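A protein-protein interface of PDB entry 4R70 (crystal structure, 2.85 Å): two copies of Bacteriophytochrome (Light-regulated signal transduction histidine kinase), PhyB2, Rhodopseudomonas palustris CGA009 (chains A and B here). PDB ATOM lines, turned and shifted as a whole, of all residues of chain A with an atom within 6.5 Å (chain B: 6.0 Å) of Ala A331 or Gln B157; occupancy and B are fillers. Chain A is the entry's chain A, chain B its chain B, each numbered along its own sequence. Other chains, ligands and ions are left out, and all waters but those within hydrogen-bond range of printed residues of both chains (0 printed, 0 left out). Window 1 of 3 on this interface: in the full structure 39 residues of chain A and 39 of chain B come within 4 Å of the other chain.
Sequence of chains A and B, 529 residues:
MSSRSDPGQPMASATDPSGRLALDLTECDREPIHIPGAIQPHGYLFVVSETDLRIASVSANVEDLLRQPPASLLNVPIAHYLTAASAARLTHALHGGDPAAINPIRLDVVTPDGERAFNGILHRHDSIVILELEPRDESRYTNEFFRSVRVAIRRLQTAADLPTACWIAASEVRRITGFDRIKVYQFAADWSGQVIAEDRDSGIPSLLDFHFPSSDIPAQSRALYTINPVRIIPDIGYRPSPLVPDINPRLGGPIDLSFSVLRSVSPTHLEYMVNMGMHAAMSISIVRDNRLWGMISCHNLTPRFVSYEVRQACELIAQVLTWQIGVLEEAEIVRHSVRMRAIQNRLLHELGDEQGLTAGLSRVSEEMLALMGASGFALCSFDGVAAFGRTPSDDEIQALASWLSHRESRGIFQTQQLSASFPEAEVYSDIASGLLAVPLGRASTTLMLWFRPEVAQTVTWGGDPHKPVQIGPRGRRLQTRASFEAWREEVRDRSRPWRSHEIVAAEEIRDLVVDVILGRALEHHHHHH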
ATOM      1  N   GLN A 157     -12.796 -14.787 -20.428  1.00  0.00           N
ATOM      2  CA  GLN A 157     -13.425 -14.873 -19.138  1.00  0.00           C
ATOM      3  C   GLN A 157     -14.292 -13.631 -18.828  1.00  0.00           C
ATOM      4  O   GLN A 157     -15.327 -13.706 -18.164  1.00  0.00           O
ATOM      5  CB  GLN A 157     -12.321 -14.968 -18.173  1.00  0.00           C
ATOM      6  CG  GLN A 157     -11.771 -16.290 -17.971  1.00  0.00           C
ATOM      7  CD  GLN A 157     -10.532 -16.285 -17.049  1.00  0.00           C
ATOM      8  OE1 GLN A 157      -9.898 -15.232 -16.789  1.00  0.00           O
ATOM      9  NE2 GLN A 157     -10.154 -17.466 -16.611  1.00  0.00           N
ATOM     10  N   THR A 158     -13.900 -12.500 -19.358  1.00  0.00           N
ATOM     11  CA  THR A 158     -14.673 -11.341 -19.211  1.00  0.00           C
ATOM     12  C   THR A 158     -15.715 -11.184 -20.302  1.00  0.00           C
ATOM     13  O   THR A 158     -16.226 -10.130 -20.456  1.00  0.00           O
ATOM     14  CB  THR A 158     -13.782 -10.173 -19.263  1.00  0.00           C
ATOM     15  OG1 THR A 158     -12.906 -10.296 -20.389  1.00  0.00           O
ATOM     16  CG2 THR A 158     -12.989 -10.109 -17.969  1.00  0.00           C
ATOM     17  N   ALA A 159     -16.014 -12.193 -21.090  1.00  0.00           N
ATOM     18  CA  ALA A 159     -17.109 -12.071 -22.070  1.00  0.00           C
ATOM     19  C   ALA A 159     -18.462 -11.796 -21.493  1.00  0.00           C
ATOM     20  O   ALA A 159     -18.839 -12.327 -20.473  1.00  0.00           O
ATOM     21  CB  ALA A 159     -17.261 -13.311 -22.990  1.00  0.00           C
ATOM     22  N   GLY A 326     -20.671 -22.728 -18.342  1.00  0.00           N
ATOM     23  CA  GLY A 326     -21.347 -22.645 -17.082  1.00  0.00           C
ATOM     24  C   GLY A 326     -21.250 -21.345 -16.272  1.00  0.00           C
ATOM     25  O   GLY A 326     -22.203 -20.932 -15.687  1.00  0.00           O
ATOM     26  N   VAL A 327     -20.135 -20.645 -16.247  1.00  0.00           N
ATOM     27  CA  VAL A 327     -20.165 -19.444 -15.436  1.00  0.00           C
ATOM     28  C   VAL A 327     -21.138 -18.471 -16.041  1.00  0.00           C
ATOM     29  O   VAL A 327     -21.886 -17.838 -15.336  1.00  0.00           O
ATOM     30  CB  VAL A 327     -18.772 -18.787 -15.045  1.00  0.00           C
ATOM     31  CG1 VAL A 327     -17.588 -19.640 -15.263  1.00  0.00           C
ATOM     32  CG2 VAL A 327     -18.623 -17.449 -15.602  1.00  0.00           C
ATOM     33  N   LEU A 328     -21.192 -18.453 -17.364  1.00  0.00           N
ATOM     34  CA  LEU A 328     -22.094 -17.605 -18.043  1.00  0.00           C
ATOM     35  C   LEU A 328     -23.533 -17.892 -17.644  1.00  0.00           C
ATOM     36  O   LEU A 328     -24.272 -16.958 -17.367  1.00  0.00           O
ATOM     37  CB  LEU A 328     -21.895 -17.765 -19.495  1.00  0.00           C
ATOM     38  CG  LEU A 328     -20.803 -16.881 -20.103  1.00  0.00           C
ATOM     39  CD1 LEU A 328     -20.661 -17.214 -21.491  1.00  0.00           C
ATOM     40  CD2 LEU A 328     -21.191 -15.460 -20.060  1.00  0.00           C
ATOM     41  N   GLU A 329     -23.890 -19.172 -17.546  1.00  0.00           N
ATOM     42  CA  GLU A 329     -25.236 -19.653 -17.210  1.00  0.00           C
ATOM     43  C   GLU A 329     -25.608 -19.134 -15.827  1.00  0.00           C
ATOM     44  O   GLU A 329     -26.566 -18.380 -15.629  1.00  0.00           O
ATOM     45  CB  GLU A 329     -25.257 -21.158 -17.195  1.00  0.00           C
ATOM     46  CG  GLU A 329     -25.731 -21.940 -18.439  1.00  0.00           C
ATOM     47  CD  GLU A 329     -25.575 -23.522 -18.363  1.00  0.00           C
ATOM     48  OE1 GLU A 329     -25.329 -24.133 -17.304  1.00  0.00           O
ATOM     49  OE2 GLU A 329     -25.680 -24.168 -19.418  1.00  0.00           O
ATOM     50  N   GLU A 330     -24.773 -19.486 -14.861  1.00  0.00           N
ATOM     51  CA  GLU A 330     -24.939 -18.966 -13.526  1.00  0.00           C
ATOM     52  C   GLU A 330     -25.113 -17.462 -13.503  1.00  0.00           C
ATOM     53  O   GLU A 330     -26.065 -16.956 -12.945  1.00  0.00           O
ATOM     54  CB  GLU A 330     -23.786 -19.376 -12.672  1.00  0.00           C
ATOM     55  CG  GLU A 330     -23.653 -20.857 -12.519  1.00  0.00           C
ATOM     56  CD  GLU A 330     -22.353 -21.366 -11.745  1.00  0.00           C
ATOM     57  OE1 GLU A 330     -22.015 -20.919 -10.599  1.00  0.00           O
ATOM     58  OE2 GLU A 330     -21.619 -22.210 -12.339  1.00  0.00           O
ATOM     59  N   ALA A 331     -24.215 -16.759 -14.170  1.00  0.00           N
ATOM     60  CA  ALA A 331     -24.336 -15.315 -14.236  1.00  0.00           C
ATOM     61  C   ALA A 331     -25.664 -14.893 -14.796  1.00  0.00           C
ATOM     62  O   ALA A 331     -26.206 -13.889 -14.370  1.00  0.00           O
ATOM     63  CB  ALA A 331     -23.242 -14.701 -15.015  1.00  0.00           C
ATOM     64  N   GLU A 332     -26.199 -15.635 -15.761  1.00  0.00           N
ATOM     65  CA  GLU A 332     -27.430 -15.162 -16.374  1.00  0.00           C
ATOM     66  C   GLU A 332     -28.512 -15.301 -15.297  1.00  0.00           C
ATOM     67  O   GLU A 332     -29.323 -14.440 -15.154  1.00  0.00           O
ATOM     68  CB  GLU A 332     -27.770 -15.839 -17.746  1.00  0.00           C
ATOM     69  CG  GLU A 332     -29.053 -15.281 -18.260  1.00  0.00           C
ATOM     70  CD  GLU A 332     -29.014 -14.863 -19.713  1.00  0.00           C
ATOM     71  OE1 GLU A 332     -28.658 -15.764 -20.542  1.00  0.00           O
ATOM     72  OE2 GLU A 332     -29.300 -13.629 -19.986  1.00  0.00           O
ATOM     73  N   ILE A 333     -28.463 -16.324 -14.456  1.00  0.00           N
ATOM     74  CA  ILE A 333     -29.438 -16.400 -13.403  1.00  0.00           C
ATOM     75  C   ILE A 333     -29.455 -15.276 -12.375  1.00  0.00           C
ATOM     76  O   ILE A 333     -30.515 -14.774 -11.982  1.00  0.00           O
ATOM     77  CB  ILE A 333     -29.256 -17.667 -12.632  1.00  0.00           C
ATOM     78  CG1 ILE A 333     -29.818 -18.819 -13.467  1.00  0.00           C
ATOM     79  CG2 ILE A 333     -30.032 -17.639 -11.427  1.00  0.00           C
ATOM     80  CD1 ILE A 333     -29.047 -20.018 -13.132  1.00  0.00           C
ATOM     81  N   VAL A 334     -28.278 -14.875 -11.958  1.00  0.00           N
ATOM     82  CA  VAL A 334     -28.109 -13.919 -10.862  1.00  0.00           C
ATOM     83  C   VAL A 334     -28.697 -12.625 -11.300  1.00  0.00           C
ATOM     84  O   VAL A 334     -29.363 -11.938 -10.543  1.00  0.00           O
ATOM     85  CB  VAL A 334     -26.628 -13.819 -10.488  1.00  0.00           C
ATOM     86  CG1 VAL A 334     -26.313 -12.726  -9.571  1.00  0.00           C
ATOM     87  CG2 VAL A 334     -26.179 -15.089  -9.870  1.00  0.00           C
ATOM     88  N   ARG A 335     -28.464 -12.343 -12.574  1.00  0.00           N
ATOM     89  CA  ARG A 335     -28.968 -11.170 -13.255  1.00  0.00           C
ATOM     90  C   ARG A 335     -30.467 -11.111 -13.253  1.00  0.00           C
ATOM     91  O   ARG A 335     -31.034 -10.155 -13.674  1.00  0.00           O
ATOM     92  CB  ARG A 335     -28.481 -11.145 -14.700  1.00  0.00           C
ATOM     93  CG  ARG A 335     -27.016 -10.710 -14.763  1.00  0.00           C
ATOM     94  CD  ARG A 335     -26.722  -9.901 -15.976  1.00  0.00           C
ATOM     95  NE  ARG A 335     -26.954 -10.756 -17.102  1.00  0.00           N
ATOM     96  CZ  ARG A 335     -26.062 -11.609 -17.548  1.00  0.00           C
ATOM     97  NH1 ARG A 335     -24.837 -11.643 -17.016  1.00  0.00           N
ATOM     98  NH2 ARG A 335     -26.398 -12.359 -18.575  1.00  0.00           N
ATOM     99  N   HIS A 336     -31.128 -12.171 -12.872  1.00  0.00           N
ATOM    100  CA  HIS A 336     -32.547 -12.145 -13.006  1.00  0.00           C
ATOM    101  C   HIS A 336     -33.226 -12.383 -11.686  1.00  0.00           C
ATOM    102  O   HIS A 336     -34.414 -12.697 -11.629  1.00  0.00           O
ATOM    103  CB  HIS A 336     -32.978 -13.106 -14.082  1.00  0.00           C
ATOM    104  CG  HIS A 336     -32.623 -12.646 -15.472  1.00  0.00           C
ATOM    105  ND1 HIS A 336     -32.362 -13.485 -16.501  1.00  0.00           N
ATOM    106  CD2 HIS A 336     -32.458 -11.371 -15.944  1.00  0.00           C
ATOM    107  CE1 HIS A 336     -32.072 -12.792 -17.591  1.00  0.00           C
ATOM    108  NE2 HIS A 336     -32.117 -11.500 -17.270  1.00  0.00           N
ATOM    109  N   ALA B 152     -25.983  -3.278 -13.809  1.00  0.00           N
ATOM    110  CA  ALA B 152     -24.985  -3.111 -12.784  1.00  0.00           C
ATOM    111  C   ALA B 152     -24.261  -4.443 -12.656  1.00  0.00           C
ATOM    112  O   ALA B 152     -23.048  -4.563 -12.844  1.00  0.00           O
ATOM    113  CB  ALA B 152     -25.650  -2.686 -11.463  1.00  0.00           C
ATOM    114  N   ILE B 153     -25.069  -5.463 -12.467  1.00  0.00           N
ATOM    115  CA  ILE B 153     -24.582  -6.753 -12.179  1.00  0.00           C
ATOM    116  C   ILE B 153     -23.761  -7.345 -13.296  1.00  0.00           C
ATOM    117  O   ILE B 153     -22.725  -7.945 -13.058  1.00  0.00           O
ATOM    118  CB  ILE B 153     -25.751  -7.660 -11.909  1.00  0.00           C
ATOM    119  CG1 ILE B 153     -26.484  -7.244 -10.619  1.00  0.00           C
ATOM    120  CG2 ILE B 153     -25.259  -9.063 -11.833  1.00  0.00           C
ATOM    121  CD1 ILE B 153     -27.724  -8.034 -10.433  1.00  0.00           C
ATOM    122  N   ARG B 154     -24.251  -7.229 -14.521  1.00  0.00           N
ATOM    123  CA  ARG B 154     -23.467  -7.645 -15.644  1.00  0.00           C
ATOM    124  C   ARG B 154     -22.085  -7.044 -15.600  1.00  0.00           C
ATOM    125  O   ARG B 154     -21.086  -7.721 -15.757  1.00  0.00           O
ATOM    126  CB  ARG B 154     -24.106  -7.249 -16.949  1.00  0.00           C
ATOM    127  CG  ARG B 154     -23.317  -7.715 -18.225  1.00  0.00           C
ATOM    128  CD  ARG B 154     -23.826  -7.164 -19.601  1.00  0.00           C
ATOM    129  NE  ARG B 154     -25.211  -7.562 -19.833  1.00  0.00           N
ATOM    130  CZ  ARG B 154     -25.595  -8.788 -20.166  1.00  0.00           C
ATOM    131  NH1 ARG B 154     -24.705  -9.760 -20.339  1.00  0.00           N
ATOM    132  NH2 ARG B 154     -26.884  -9.026 -20.330  1.00  0.00           N
ATOM    133  N   ARG B 155     -21.980  -5.773 -15.354  1.00  0.00           N
ATOM    134  CA  ARG B 155     -20.663  -5.157 -15.494  1.00  0.00           C
ATOM    135  C   ARG B 155     -19.766  -5.812 -14.451  1.00  0.00           C
ATOM    136  O   ARG B 155     -18.634  -6.155 -14.667  1.00  0.00           O
ATOM    137  CB  ARG B 155     -20.755  -3.656 -15.274  1.00  0.00           C
ATOM    138  CG  ARG B 155     -21.539  -2.909 -16.322  1.00  0.00           C
ATOM    139  CD  ARG B 155     -21.608  -1.430 -15.973  1.00  0.00           C
ATOM    140  NE  ARG B 155     -22.615  -0.667 -16.710  1.00  0.00           N
ATOM    141  CZ  ARG B 155     -22.742   0.659 -16.613  1.00  0.00           C
ATOM    142  NH1 ARG B 155     -21.944   1.370 -15.812  1.00  0.00           N
ATOM    143  NH2 ARG B 155     -23.656   1.286 -17.325  1.00  0.00           N
ATOM    144  N   LEU B 156     -20.318  -5.992 -13.304  1.00  0.00           N
ATOM    145  CA  LEU B 156     -19.587  -6.464 -12.190  1.00  0.00           C
ATOM    146  C   LEU B 156     -19.059  -7.860 -12.457  1.00  0.00           C
ATOM    147  O   LEU B 156     -17.946  -8.262 -12.119  1.00  0.00           O
ATOM    148  CB  LEU B 156     -20.595  -6.526 -11.049  1.00  0.00           C
ATOM    149  CG  LEU B 156     -19.871  -6.625  -9.742  1.00  0.00           C
ATOM    150  CD1 LEU B 156     -18.620  -5.838  -9.722  1.00  0.00           C
ATOM    151  CD2 LEU B 156     -20.700  -6.211  -8.677  1.00  0.00           C
ATOM    152  N   GLN B 157     -19.883  -8.606 -13.136  1.00  0.00           N
ATOM    153  CA  GLN B 157     -19.600  -9.976 -13.330  1.00  0.00           C
ATOM    154  C   GLN B 157     -18.539 -10.119 -14.410  1.00  0.00           C
ATOM    155  O   GLN B 157     -17.678 -10.991 -14.382  1.00  0.00           O
ATOM    156  CB  GLN B 157     -20.885 -10.609 -13.804  1.00  0.00           C
ATOM    157  CG  GLN B 157     -21.879 -10.976 -12.779  1.00  0.00           C
ATOM    158  CD  GLN B 157     -23.162 -11.496 -13.380  1.00  0.00           C
ATOM    159  OE1 GLN B 157     -23.488 -11.246 -14.566  1.00  0.00           O
ATOM    160  NE2 GLN B 157     -23.910 -12.254 -12.572  1.00  0.00           N
ATOM    161  N   THR B 158     -18.566  -9.195 -15.338  1.00  0.00           N
ATOM    162  CA  THR B 158     -17.555  -9.168 -16.409  1.00  0.00           C
ATOM    163  C   THR B 158     -16.332  -8.361 -16.065  1.00  0.00           C
ATOM    164  O   THR B 158     -15.562  -8.104 -16.914  1.00  0.00           O
ATOM    165  CB  THR B 158     -18.107  -8.478 -17.660  1.00  0.00           C
ATOM    166  OG1 THR B 158     -18.790  -7.306 -17.233  1.00  0.00           O
ATOM    167  CG2 THR B 158     -19.100  -9.323 -18.368  1.00  0.00           C
ATOM    168  N   ALA B 159     -16.197  -7.924 -14.845  1.00  0.00           N
ATOM    169  CA  ALA B 159     -14.981  -7.262 -14.430  1.00  0.00           C
ATOM    170  C   ALA B 159     -13.751  -8.162 -14.551  1.00  0.00           C
ATOM    171  O   ALA B 159     -13.758  -9.365 -14.163  1.00  0.00           O
ATOM    172  CB  ALA B 159     -15.132  -6.756 -12.993  1.00  0.00           C
ATOM    173  N   VAL B 320     -23.207  -9.955  -5.108  1.00  0.00           N
ATOM    174  CA  VAL B 320     -22.651 -10.412  -6.306  1.00  0.00           C
ATOM    175  C   VAL B 320     -21.153 -10.163  -6.259  1.00  0.00           C
ATOM    176  O   VAL B 320     -20.309 -11.025  -6.574  1.00  0.00           O
ATOM    177  CB  VAL B 320     -23.262  -9.666  -7.406  1.00  0.00           C
ATOM    178  CG1 VAL B 320     -22.412  -9.816  -8.587  1.00  0.00           C
ATOM    179  CG2 VAL B 320     -24.545 -10.162  -7.663  1.00  0.00           C
ATOM    180  N   GLN B 324     -18.188 -12.715  -6.937  1.00  0.00           N
ATOM    181  CA  GLN B 324     -17.151 -12.475  -7.863  1.00  0.00           C
ATOM    182  C   GLN B 324     -15.801 -12.614  -7.338  1.00  0.00           C
ATOM    183  O   GLN B 324     -14.885 -12.992  -8.072  1.00  0.00           O
ATOM    184  CB  GLN B 324     -17.244 -11.082  -8.452  1.00  0.00           C
ATOM    185  CG  GLN B 324     -18.379 -11.031  -9.362  1.00  0.00           C
ATOM    186  CD  GLN B 324     -18.437 -12.227 -10.325  1.00  0.00           C
ATOM    187  OE1 GLN B 324     -19.397 -12.986 -10.304  1.00  0.00           O
ATOM    188  NE2 GLN B 324     -17.436 -12.363 -11.186  1.00  0.00           N
ATOM    189  N   VAL B 327     -14.688 -15.916  -8.080  1.00  0.00           N
ATOM    190  CA  VAL B 327     -14.533 -16.312  -9.425  1.00  0.00           C
ATOM    191  C   VAL B 327     -13.298 -15.572  -9.948  1.00  0.00           C
ATOM    192  O   VAL B 327     -12.472 -16.105 -10.699  1.00  0.00           O
ATOM    193  CB  VAL B 327     -15.857 -16.246 -10.302  1.00  0.00           C
ATOM    194  CG1 VAL B 327     -16.939 -15.894  -9.514  1.00  0.00           C
ATOM    195  CG2 VAL B 327     -15.736 -15.367 -11.496  1.00  0.00           C
ATOM    196  N   LEU B 328     -13.107 -14.340  -9.541  1.00  0.00           N
ATOM    197  CA  LEU B 328     -11.876 -13.759 -10.005  1.00  0.00           C
ATOM    198  C   LEU B 328     -10.701 -14.537  -9.521  1.00  0.00           C
ATOM    199  O   LEU B 328      -9.727 -14.642 -10.218  1.00  0.00           O
ATOM    200  CB  LEU B 328     -11.767 -12.343  -9.589  1.00  0.00           C
ATOM    201  CG  LEU B 328     -12.210 -11.204 -10.470  1.00  0.00           C
ATOM    202  CD1 LEU B 328     -13.021 -11.754 -11.589  1.00  0.00           C
ATOM    203  CD2 LEU B 328     -12.978 -10.238  -9.632  1.00  0.00           C
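Printed residues of chain A that touch a printed residue of chain B: Thr A158, Ala A159, Ala A331, Val A334 and Arg A335.
Hydrophobic or aromatic side chains of chain A that line the printed part of chain B: Ala A331 and Val A334.
Printed residues of chain B that touch a printed residue of chain A: Ile B153, Arg B154, Gln B157, Thr B158, Ala B159 and Val B320.
Hydrophobic or aromatic side chains of chain B that line the printed part of chain A: Ile B153 and Val B320.
CG2 of Thr A158 touches O of Thr B158, 3.4 Å away.
O of Ala B159 touches CG2 of Thr A158 (3.95 Å).
Ala A159 touches Thr B158.
Gln B157 touches Val A334.
Val A334 touches Val B320 (CG1 to CG2, 3.7 Å).
Arg A335 touches Ile B153.
NH1 of Arg B154 touches NH2 of Arg A335, at 3.6 Å.
Printed residues of chain B within 4 Å of Ala A331: Gln B157 (3.3 Å).
Of the printed residues of chain A, Val B320 touches Val A334 (3.7 Å).
Printed residues of chain A within 4 Å of Arg B154: Arg A335 (3.6 Å).
Printed residues of chain B within 4 Å of Ala A159: Thr B158 (3.7 Å).
Of the printed residues of chain A, Ile B153 touches Arg A335.
The nearest residue of chain B that does not touch Ala A331 is Ile B153 (5.5 Å).
The nearest printed residue of chain A that does not touch Gln B157 is Glu A332 (5.2 Å).
NE2 of Gln B157 sits at hydrogen-bond distance from O of Ala A331 (3.3 Å).
NH1 of Arg A335 lies within hydrogen-bond range of OE1 of Gln B157 (2.8 Å).
Thr B158 touches its own counterpart, Thr A158.
Thr A158 touches Ala B159, and with the chains exchanged Ala A159 touches Thr B158.
Positions printed for both chains: 157, 158, 159, 327 and 328.
NH2 of Arg A335 is in salt-bridge range of OE2 of Glu A332 (3.5 Å).
The side-chain hydroxyl (OG1) of Thr B158 sits at hydrogen-bond distance from the backbone carbonyl oxygen (O) of Arg B154 (2.8 Å).
The backbone carbonyl oxygen (O) of Arg B155 sits at hydrogen-bond distance from the side-chain hydroxyl (OG1) of Thr B158 (2.8 Å).
O of Gln B157 sits at hydrogen-bond distance from NE2 of Gln B324 (3.5 Å).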
